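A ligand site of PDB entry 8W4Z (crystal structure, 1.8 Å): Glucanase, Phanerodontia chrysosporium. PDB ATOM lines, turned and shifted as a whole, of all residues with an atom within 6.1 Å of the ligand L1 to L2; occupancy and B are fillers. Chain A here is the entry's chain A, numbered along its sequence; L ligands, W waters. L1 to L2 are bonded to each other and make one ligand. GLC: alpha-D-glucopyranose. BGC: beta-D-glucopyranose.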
ATOM      1  N   TYR A  83     -22.977  30.807   3.995  1.00  0.00           N
ATOM      2  CA  TYR A  83     -23.006  30.865   5.470  1.00  0.00           C
ATOM      3  C   TYR A  83     -22.312  32.134   5.943  1.00  0.00           C
ATOM      4  O   TYR A  83     -21.186  32.093   6.453  1.00  0.00           O
ATOM      5  CB  TYR A  83     -22.328  29.621   6.038  1.00  0.00           C
ATOM      6  CG  TYR A  83     -22.396  29.433   7.553  1.00  0.00           C
ATOM      7  CD1 TYR A  83     -23.594  29.309   8.199  1.00  0.00           C
ATOM      8  CD2 TYR A  83     -21.236  29.379   8.303  1.00  0.00           C
ATOM      9  CE1 TYR A  83     -23.644  29.130   9.543  1.00  0.00           C
ATOM     10  CE2 TYR A  83     -21.282  29.172   9.665  1.00  0.00           C
ATOM     11  CZ  TYR A  83     -22.479  29.052  10.288  1.00  0.00           C
ATOM     12  OH  TYR A  83     -22.557  28.841  11.644  1.00  0.00           O
ATOM     13  N   ASP A  89     -25.403  32.477  13.664  1.00  0.00           N
ATOM     14  CA  ASP A  89     -25.318  31.525  14.780  1.00  0.00           C
ATOM     15  C   ASP A  89     -25.940  32.129  16.036  1.00  0.00           C
ATOM     16  O   ASP A  89     -25.329  32.154  17.118  1.00  0.00           O
ATOM     17  CB  ASP A  89     -23.866  31.125  14.993  1.00  0.00           C
ATOM     18  CG  ASP A  89     -23.704  29.816  15.721  1.00  0.00           C
ATOM     19  OD1 ASP A  89     -24.556  28.920  15.588  1.00  0.00           O
ATOM     20  OD2 ASP A  89     -22.665  29.654  16.407  1.00  0.00           O
ATOM     21  N   ALA A  91     -28.171  31.488  18.262  1.00  0.00           N
ATOM     22  CA  ALA A  91     -28.447  30.776  19.503  1.00  0.00           C
ATOM     23  C   ALA A  91     -27.208  30.177  20.134  1.00  0.00           C
ATOM     24  O   ALA A  91     -27.328  29.377  21.061  1.00  0.00           O
ATOM     25  CB  ALA A  91     -29.477  29.668  19.267  1.00  0.00           C
ATOM     26  N   ALA A  92     -26.026  30.475  19.598  1.00  0.00           N
ATOM     27  CA  ALA A  92     -24.777  29.927  20.121  1.00  0.00           C
ATOM     28  C   ALA A  92     -23.673  30.958  19.975  1.00  0.00           C
ATOM     29  O   ALA A  92     -23.888  32.065  19.495  1.00  0.00           O
ATOM     30  CB  ALA A  92     -24.402  28.637  19.387  1.00  0.00           C
ATOM     31  N   SER A  95     -19.675  30.056  16.299  1.00  0.00           N
ATOM     32  CA  SER A  95     -19.539  30.386  14.885  1.00  0.00           C
ATOM     33  C   SER A  95     -20.069  31.786  14.562  1.00  0.00           C
ATOM     34  O   SER A  95     -20.509  32.043  13.450  1.00  0.00           O
ATOM     35  CB  SER A  95     -20.211  29.335  14.007  1.00  0.00           C
ATOM     36  OG  SER A  95     -19.436  28.130  13.993  1.00  0.00           O
ATOM     37  N   ASP A 135     -28.690  26.487   9.935  1.00  0.00           N
ATOM     38  CA  ASP A 135     -29.175  26.846  11.267  1.00  0.00           C
ATOM     39  C   ASP A 135     -30.130  28.028  11.314  1.00  0.00           C
ATOM     40  O   ASP A 135     -30.896  28.160  12.265  1.00  0.00           O
ATOM     41  CB  ASP A 135     -27.998  27.136  12.181  1.00  0.00           C
ATOM     42  CG  ASP A 135     -27.084  25.932  12.352  1.00  0.00           C
ATOM     43  OD1 ASP A 135     -27.511  24.758  12.161  1.00  0.00           O
ATOM     44  OD2 ASP A 135     -25.905  26.176  12.602  1.00  0.00           O
ATOM     45  N   ASN A 139     -33.430  28.174  13.716  1.00  0.00           N
ATOM     46  CA  ASN A 139     -33.400  29.052  14.899  1.00  0.00           C
ATOM     47  C   ASN A 139     -34.645  29.929  14.984  1.00  0.00           C
ATOM     48  O   ASN A 139     -35.087  30.274  16.086  1.00  0.00           O
ATOM     49  CB  ASN A 139     -32.134  29.927  14.896  1.00  0.00           C
ATOM     50  CG  ASN A 139     -30.969  29.276  15.548  1.00  0.00           C
ATOM     51  OD1 ASN A 139     -31.140  28.516  16.531  1.00  0.00           O
ATOM     52  ND2 ASN A 139     -29.765  29.574  15.063  1.00  0.00           N
ATOM     53  N   THR A 142     -37.603  27.591  16.711  1.00  0.00           N
ATOM     54  CA  THR A 142     -37.591  27.156  18.109  1.00  0.00           C
ATOM     55  C   THR A 142     -36.899  28.109  19.065  1.00  0.00           C
ATOM     56  O   THR A 142     -36.953  27.884  20.286  1.00  0.00           O
ATOM     57  CB  THR A 142     -36.906  25.775  18.256  1.00  0.00           C
ATOM     58  OG1 THR A 142     -35.507  25.921  17.992  1.00  0.00           O
ATOM     59  CG2 THR A 142     -37.521  24.788  17.387  1.00  0.00           C
ATOM     60  N   ASN A 143     -36.216  29.145  18.561  1.00  0.00           N
ATOM     61  CA  ASN A 143     -35.360  29.981  19.398  1.00  0.00           C
ATOM     62  C   ASN A 143     -35.732  31.454  19.342  1.00  0.00           C
ATOM     63  O   ASN A 143     -34.871  32.299  19.530  1.00  0.00           O
ATOM     64  CB  ASN A 143     -33.891  29.794  19.041  1.00  0.00           C
ATOM     65  CG  ASN A 143     -33.279  28.603  19.736  1.00  0.00           C
ATOM     66  OD1 ASN A 143     -33.611  28.303  20.880  1.00  0.00           O
ATOM     67  ND2 ASN A 143     -32.362  27.924  19.045  1.00  0.00           N
ATOM     68  N   HIS A 180     -32.592  19.403  11.851  1.00  0.00           N
ATOM     69  CA  HIS A 180     -32.474  17.945  11.896  1.00  0.00           C
ATOM     70  C   HIS A 180     -33.581  17.368  12.781  1.00  0.00           C
ATOM     71  O   HIS A 180     -34.376  18.096  13.375  1.00  0.00           O
ATOM     72  CB  HIS A 180     -31.102  17.482  12.373  1.00  0.00           C
ATOM     73  CG  HIS A 180     -30.753  17.916  13.762  1.00  0.00           C
ATOM     74  ND1 HIS A 180     -31.193  17.263  14.887  1.00  0.00           N
ATOM     75  CD2 HIS A 180     -29.959  18.925  14.193  1.00  0.00           C
ATOM     76  CE1 HIS A 180     -30.726  17.874  15.957  1.00  0.00           C
ATOM     77  NE2 HIS A 180     -29.974  18.885  15.568  1.00  0.00           N
ATOM     78  N   GLY A 182     -33.784  16.023  15.666  1.00  0.00           N
ATOM     79  CA  GLY A 182     -33.829  16.404  17.065  1.00  0.00           C
ATOM     80  C   GLY A 182     -34.114  17.859  17.308  1.00  0.00           C
ATOM     81  O   GLY A 182     -34.239  18.274  18.466  1.00  0.00           O
ATOM     82  N   TRP A 183     -34.214  18.659  16.245  1.00  0.00           N
ATOM     83  CA  TRP A 183     -34.491  20.080  16.340  1.00  0.00           C
ATOM     84  C   TRP A 183     -35.923  20.386  15.828  1.00  0.00           C
ATOM     85  O   TRP A 183     -36.789  20.758  16.609  1.00  0.00           O
ATOM     86  CB  TRP A 183     -33.446  20.816  15.511  1.00  0.00           C
ATOM     87  CG  TRP A 183     -33.316  22.289  15.751  1.00  0.00           C
ATOM     88  CD1 TRP A 183     -34.180  23.102  16.432  1.00  0.00           C
ATOM     89  CD2 TRP A 183     -32.239  23.115  15.321  1.00  0.00           C
ATOM     90  NE1 TRP A 183     -33.700  24.385  16.453  1.00  0.00           N
ATOM     91  CE2 TRP A 183     -32.512  24.427  15.779  1.00  0.00           C
ATOM     92  CE3 TRP A 183     -31.058  22.881  14.609  1.00  0.00           C
ATOM     93  CZ2 TRP A 183     -31.662  25.483  15.546  1.00  0.00           C
ATOM     94  CZ3 TRP A 183     -30.208  23.936  14.376  1.00  0.00           C
ATOM     95  CH2 TRP A 183     -30.510  25.216  14.845  1.00  0.00           C
ATOM     96  N   ASN A 216     -29.685  17.681   8.793  1.00  0.00           N
ATOM     97  CA  ASN A 216     -28.570  17.106   9.554  1.00  0.00           C
ATOM     98  C   ASN A 216     -27.226  17.746   9.253  1.00  0.00           C
ATOM     99  O   ASN A 216     -26.189  17.158   9.546  1.00  0.00           O
ATOM    100  CB  ASN A 216     -28.453  15.595   9.311  1.00  0.00           C
ATOM    101  CG  ASN A 216     -27.772  14.850  10.450  1.00  0.00           C
ATOM    102  OD1 ASN A 216     -28.092  15.055  11.610  1.00  0.00           O
ATOM    103  ND2 ASN A 216     -26.829  13.945  10.099  1.00  0.00           N
ATOM    104  N   VAL A 217     -27.246  18.946   8.667  1.00  0.00           N
ATOM    105  CA  VAL A 217     -26.014  19.638   8.342  1.00  0.00           C
ATOM    106  C   VAL A 217     -25.221  19.880   9.617  1.00  0.00           C
ATOM    107  O   VAL A 217     -25.712  20.504  10.575  1.00  0.00           O
ATOM    108  CB  VAL A 217     -26.301  20.940   7.596  1.00  0.00           C
ATOM    109  CG1 VAL A 217     -25.033  21.726   7.367  1.00  0.00           C
ATOM    110  CG2 VAL A 217     -26.940  20.620   6.255  1.00  0.00           C
ATOM    111  N   ALA A 218     -23.956  19.451   9.616  1.00  0.00           N
ATOM    112  CA  ALA A 218     -23.056  19.597  10.762  1.00  0.00           C
ATOM    113  C   ALA A 218     -23.524  18.816  11.977  1.00  0.00           C
ATOM    114  O   ALA A 218     -23.015  19.011  13.083  1.00  0.00           O
ATOM    115  CB  ALA A 218     -22.860  21.069  11.122  1.00  0.00           C
ATOM    116  N   ASN A 219     -24.476  17.894  11.818  1.00  0.00           N
ATOM    117  CA  ASN A 219     -24.901  17.089  12.952  1.00  0.00           C
ATOM    118  C   ASN A 219     -24.558  15.617  12.698  1.00  0.00           C
ATOM    119  O   ASN A 219     -23.753  15.297  11.826  1.00  0.00           O
ATOM    120  CB  ASN A 219     -26.377  17.293  13.253  1.00  0.00           C
ATOM    121  CG  ASN A 219     -26.683  17.187  14.747  1.00  0.00           C
ATOM    122  OD1 ASN A 219     -26.810  16.068  15.273  1.00  0.00           O
ATOM    123  ND2 ASN A 219     -26.732  18.339  15.457  1.00  0.00           N
ATOM    124  N   ARG A 273     -23.698  10.424  22.125  1.00  0.00           N
ATOM    125  CA  ARG A 273     -23.992  11.675  22.790  1.00  0.00           C
ATOM    126  C   ARG A 273     -24.740  11.425  24.093  1.00  0.00           C
ATOM    127  O   ARG A 273     -25.472  10.442  24.233  1.00  0.00           O
ATOM    128  CB  ARG A 273     -24.819  12.598  21.886  1.00  0.00           C
ATOM    129  CG  ARG A 273     -24.045  13.228  20.767  1.00  0.00           C
ATOM    130  CD  ARG A 273     -24.963  13.996  19.841  1.00  0.00           C
ATOM    131  NE  ARG A 273     -25.764  13.132  18.986  1.00  0.00           N
ATOM    132  CZ  ARG A 273     -26.567  13.573  18.025  1.00  0.00           C
ATOM    133  NH1 ARG A 273     -26.751  14.859  17.815  1.00  0.00           N
ATOM    134  NH2 ARG A 273     -27.205  12.691  17.243  1.00  0.00           N
ATOM    135  N   TRP A 276     -29.301  15.063  23.150  1.00  0.00           N
ATOM    136  CA  TRP A 276     -29.449  15.327  21.718  1.00  0.00           C
ATOM    137  C   TRP A 276     -28.925  16.704  21.334  1.00  0.00           C
ATOM    138  O   TRP A 276     -28.454  16.901  20.206  1.00  0.00           O
ATOM    139  CB  TRP A 276     -30.931  15.205  21.306  1.00  0.00           C
ATOM    140  CG  TRP A 276     -31.108  14.714  19.938  1.00  0.00           C
ATOM    141  CD1 TRP A 276     -30.178  14.664  18.959  1.00  0.00           C
ATOM    142  CD2 TRP A 276     -32.310  14.160  19.379  1.00  0.00           C
ATOM    143  NE1 TRP A 276     -30.728  14.103  17.779  1.00  0.00           N
ATOM    144  CE2 TRP A 276     -32.030  13.764  18.045  1.00  0.00           C
ATOM    145  CE3 TRP A 276     -33.579  13.927  19.884  1.00  0.00           C
ATOM    146  CZ2 TRP A 276     -32.990  13.214  17.224  1.00  0.00           C
ATOM    147  CZ3 TRP A 276     -34.537  13.386  19.059  1.00  0.00           C
ATOM    148  CH2 TRP A 276     -34.228  13.021  17.746  1.00  0.00           C
ATOM    149  N   GLY A 277     -29.014  17.675  22.232  1.00  0.00           N
ATOM    150  CA  GLY A 277     -28.538  19.019  21.914  1.00  0.00           C
ATOM    151  C   GLY A 277     -27.036  19.214  21.970  1.00  0.00           C
ATOM    152  O   GLY A 277     -26.559  20.340  21.784  1.00  0.00           O
ATOM    153  N   ASP A 278     -26.279  18.159  22.230  1.00  0.00           N
ATOM    154  CA  ASP A 278     -24.822  18.262  22.232  1.00  0.00           C
ATOM    155  C   ASP A 278     -24.362  18.195  20.781  1.00  0.00           C
ATOM    156  O   ASP A 278     -24.433  17.127  20.185  1.00  0.00           O
ATOM    157  CB  ASP A 278     -24.173  17.126  23.033  1.00  0.00           C
ATOM    158  CG  ASP A 278     -24.627  17.095  24.479  1.00  0.00           C
ATOM    159  OD1 ASP A 278     -25.246  18.045  24.954  1.00  0.00           O
ATOM    160  OD2 ASP A 278     -24.366  16.073  25.140  1.00  0.00           O
ATOM    161  N   TRP A 279     -23.846  19.304  20.242  1.00  0.00           N
ATOM    162  CA  TRP A 279     -23.539  19.407  18.812  1.00  0.00           C
ATOM    163  C   TRP A 279     -22.062  19.623  18.521  1.00  0.00           C
ATOM    164  O   TRP A 279     -21.666  19.516  17.358  1.00  0.00           O
ATOM    165  CB  TRP A 279     -24.342  20.571  18.162  1.00  0.00           C
ATOM    166  CG  TRP A 279     -24.221  21.865  18.911  1.00  0.00           C
ATOM    167  CD1 TRP A 279     -25.113  22.376  19.812  1.00  0.00           C
ATOM    168  CD2 TRP A 279     -23.154  22.825  18.819  1.00  0.00           C
ATOM    169  NE1 TRP A 279     -24.654  23.561  20.320  1.00  0.00           N
ATOM    170  CE2 TRP A 279     -23.453  23.861  19.730  1.00  0.00           C
ATOM    171  CE3 TRP A 279     -21.961  22.895  18.096  1.00  0.00           C
ATOM    172  CZ2 TRP A 279     -22.603  24.950  19.936  1.00  0.00           C
ATOM    173  CZ3 TRP A 279     -21.116  23.969  18.285  1.00  0.00           C
ATOM    174  CH2 TRP A 279     -21.449  24.991  19.192  1.00  0.00           C
HETATM  175  C1  GLC L   1     -31.151  21.634  19.580  1.00  0.00           C
HETATM  176  C2  GLC L   1     -30.430  20.961  18.426  1.00  0.00           C
HETATM  177  C3  GLC L   1     -29.060  21.571  18.225  1.00  0.00           C
HETATM  178  C4  GLC L   1     -29.165  23.052  18.049  1.00  0.00           C
HETATM  179  C5  GLC L   1     -30.011  23.716  19.216  1.00  0.00           C
HETATM  180  C6  GLC L   1     -30.069  25.087  18.743  1.00  0.00           C
HETATM  181  O1  GLC L   1     -30.366  21.390  20.760  1.00  0.00           O
HETATM  182  O2  GLC L   1     -30.258  19.575  18.685  1.00  0.00           O
HETATM  183  O3  GLC L   1     -28.540  20.968  16.999  1.00  0.00           O
HETATM  184  O4  GLC L   1     -27.861  23.701  18.072  1.00  0.00           O
HETATM  185  O5  GLC L   1     -31.233  23.047  19.336  1.00  0.00           O
HETATM  186  O6  GLC L   1     -30.572  25.839  19.979  1.00  0.00           O
HETATM  187  C2  BGC L   2     -26.150  25.033  17.080  1.00  0.00           C
HETATM  188  C3  BGC L   2     -25.442  25.367  15.809  1.00  0.00           C
HETATM  189  C4  BGC L   2     -24.974  24.071  15.131  1.00  0.00           C
HETATM  190  C5  BGC L   2     -26.136  23.175  14.964  1.00  0.00           C
HETATM  191  C6  BGC L   2     -25.697  21.833  14.395  1.00  0.00           C
HETATM  192  C1  BGC L   2     -27.301  24.064  16.818  1.00  0.00           C
HETATM  193  O2  BGC L   2     -26.714  26.234  17.720  1.00  0.00           O
HETATM  194  O3  BGC L   2     -24.244  26.148  16.087  1.00  0.00           O
HETATM  195  O4  BGC L   2     -24.416  24.382  13.880  1.00  0.00           O
HETATM  196  O5  BGC L   2     -26.777  22.903  16.243  1.00  0.00           O
HETATM  197  O6  BGC L   2     -26.854  20.954  14.254  1.00  0.00           O
HETATM  198  C2  BGC L   3     -17.679  27.185  10.902  1.00  0.00           C
HETATM  199  C3  BGC L   3     -17.292  27.608   9.533  1.00  0.00           C
HETATM  200  C4  BGC L   3     -16.932  26.477   8.674  1.00  0.00           C
HETATM  201  C5  BGC L   3     -17.972  25.434   8.650  1.00  0.00           C
HETATM  202  C6  BGC L   3     -17.531  24.202   7.915  1.00  0.00           C
HETATM  203  C1  BGC L   3     -18.781  26.089  10.940  1.00  0.00           C
HETATM  204  O1  BGC L   3     -18.939  25.649  12.148  1.00  0.00           O
HETATM  205  O2  BGC L   3     -18.127  28.299  11.670  1.00  0.00           O
HETATM  206  O3  BGC L   3     -16.156  28.527   9.685  1.00  0.00           O
HETATM  207  O4  BGC L   3     -16.798  27.043   7.330  1.00  0.00           O
HETATM  208  O5  BGC L   3     -18.296  24.973  10.014  1.00  0.00           O
HETATM  209  O6  BGC L   3     -16.502  23.496   8.595  1.00  0.00           O
HETATM  210  O   HOH W   1     -21.360  23.121  14.168  1.00  0.00           O
HETATM  211  O   HOH W   2     -21.778  27.441  17.523  1.00  0.00           O
HETATM  212  O   HOH W   3     -27.150  28.910  16.509  1.00  0.00           O
HETATM  213  O   HOH W   4     -27.359  18.364  18.402  1.00  0.00           O
HETATM  214  O   HOH W   5     -32.083  18.244  20.063  1.00  0.00           O
HETATM  215  O   HOH W   6     -23.481  25.002  10.760  1.00  0.00           O
HETATM  216  O   HOH W   7     -33.904  24.993  20.230  1.00  0.00           O
HETATM  217  O   HOH W   8     -27.901  22.542  22.296  1.00  0.00           O
HETATM  218  O   HOH W   9     -27.467  26.358  20.432  1.00  0.00           O
HETATM  219  O   HOH W  10     -28.149  20.636  11.849  1.00  0.00           O
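The side-chain hydroxyl (OG) of Ser 95 sits at hydrogen-bond distance from an oxygen (O2) of BGC L3.
NE2 of His 180 is in hydrogen-bond range of O3 of GLC L1.
ND2 of Asn 219 is in hydrogen-bond range of O6 of BGC L2, at 2.9 Å.
An oxygen (O3) of BGC L2 sits at hydrogen-bond distance from the side-chain carboxylate (OD1) of Asp 89, at 2.8 Å.
The side-chain amide nitrogen (ND2) of Asn 143 lies within hydrogen-bond range of an oxygen (O6) of GLC L1 (2.9 Å).
The side-chain carboxylate of Asp 135 is in hydrogen-bond range of an oxygen (O4) of BGC L2 (2.7 Å).
Ala 92 touches the ligand L1 to L2.
Trp 183 touches the ligand L1 to L2.
Val 217 touches the ligand L1 to L2.
Trp 276 touches the ligand L1 to L2.
CA of Gly 277 touches O1 of GLC L1, 3.2 Å away.
CD1 of Trp 279 touches O4 of GLC L1, at 3.5 Å.
Hydrophobic or aromatic side chains that line the ligand L1 to L2: Ala 92, His 180, Trp 183 and Trp 279.
Of the 21 residues printed, 11 come within 4 Å of the ligand L1 to L2.
A ring nitrogen (NE2) of His 180 is in hydrogen-bond range of the side-chain amide nitrogen (ND2) of Asn 219, 3.3 Å away.
The backbone carbonyl oxygen of Asp 135 lies within hydrogen-bond range of the side-chain amide nitrogen of Asn 139 (3.3 Å).
The guanidinium group of Arg 273 sits at hydrogen-bond distance from the side-chain amide oxygen of Asn 219 (2.8 Å).
OD2 of Asp 89 sits at hydrogen-bond distance from N of Ser 95 (3.0 Å).
ND1 of His 180 is in hydrogen-bond range of N of Gly 182 (3.0 Å).
The side-chain amide nitrogen of Asn 143 lies within hydrogen-bond range of the side-chain amide oxygen of Asn 139, 2.9 Å away.
NE1 of Trp 183 is in hydrogen-bond range of OG1 of Thr 142 (2.8 Å).
Water W5 bridges an oxygen (O2) of GLC L1 and the backbone carbonyl oxygen (O) of Gly 182.
Water W10 lies within hydrogen-bond range of an oxygen (O6) of BGC L2 and the backbone carbonyl oxygen (O) of Val 217.
Water W9 bridges an oxygen (O2) of BGC L2 (2.8 Å) and the backbone carbonyl oxygen of Ala 91 (3.1 Å).
Water W3 lies within hydrogen-bond range of OD1 of Asp 89 (2.8 Å), O2 of BGC L2 (3.0 Å), ND2 of Asn 139 (3.1 Å) and N of Ala 91 (3.3 Å).
Water W4 lies within hydrogen-bond range of O of Trp 276 (2.6 Å), ND2 of Asn 219 (3.0 Å) and O2 of GLC L1 (3.2 Å).
Water W6 bridges the side-chain carboxylate (OD2) of Asp 135 and an oxygen (O4) of BGC L2.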
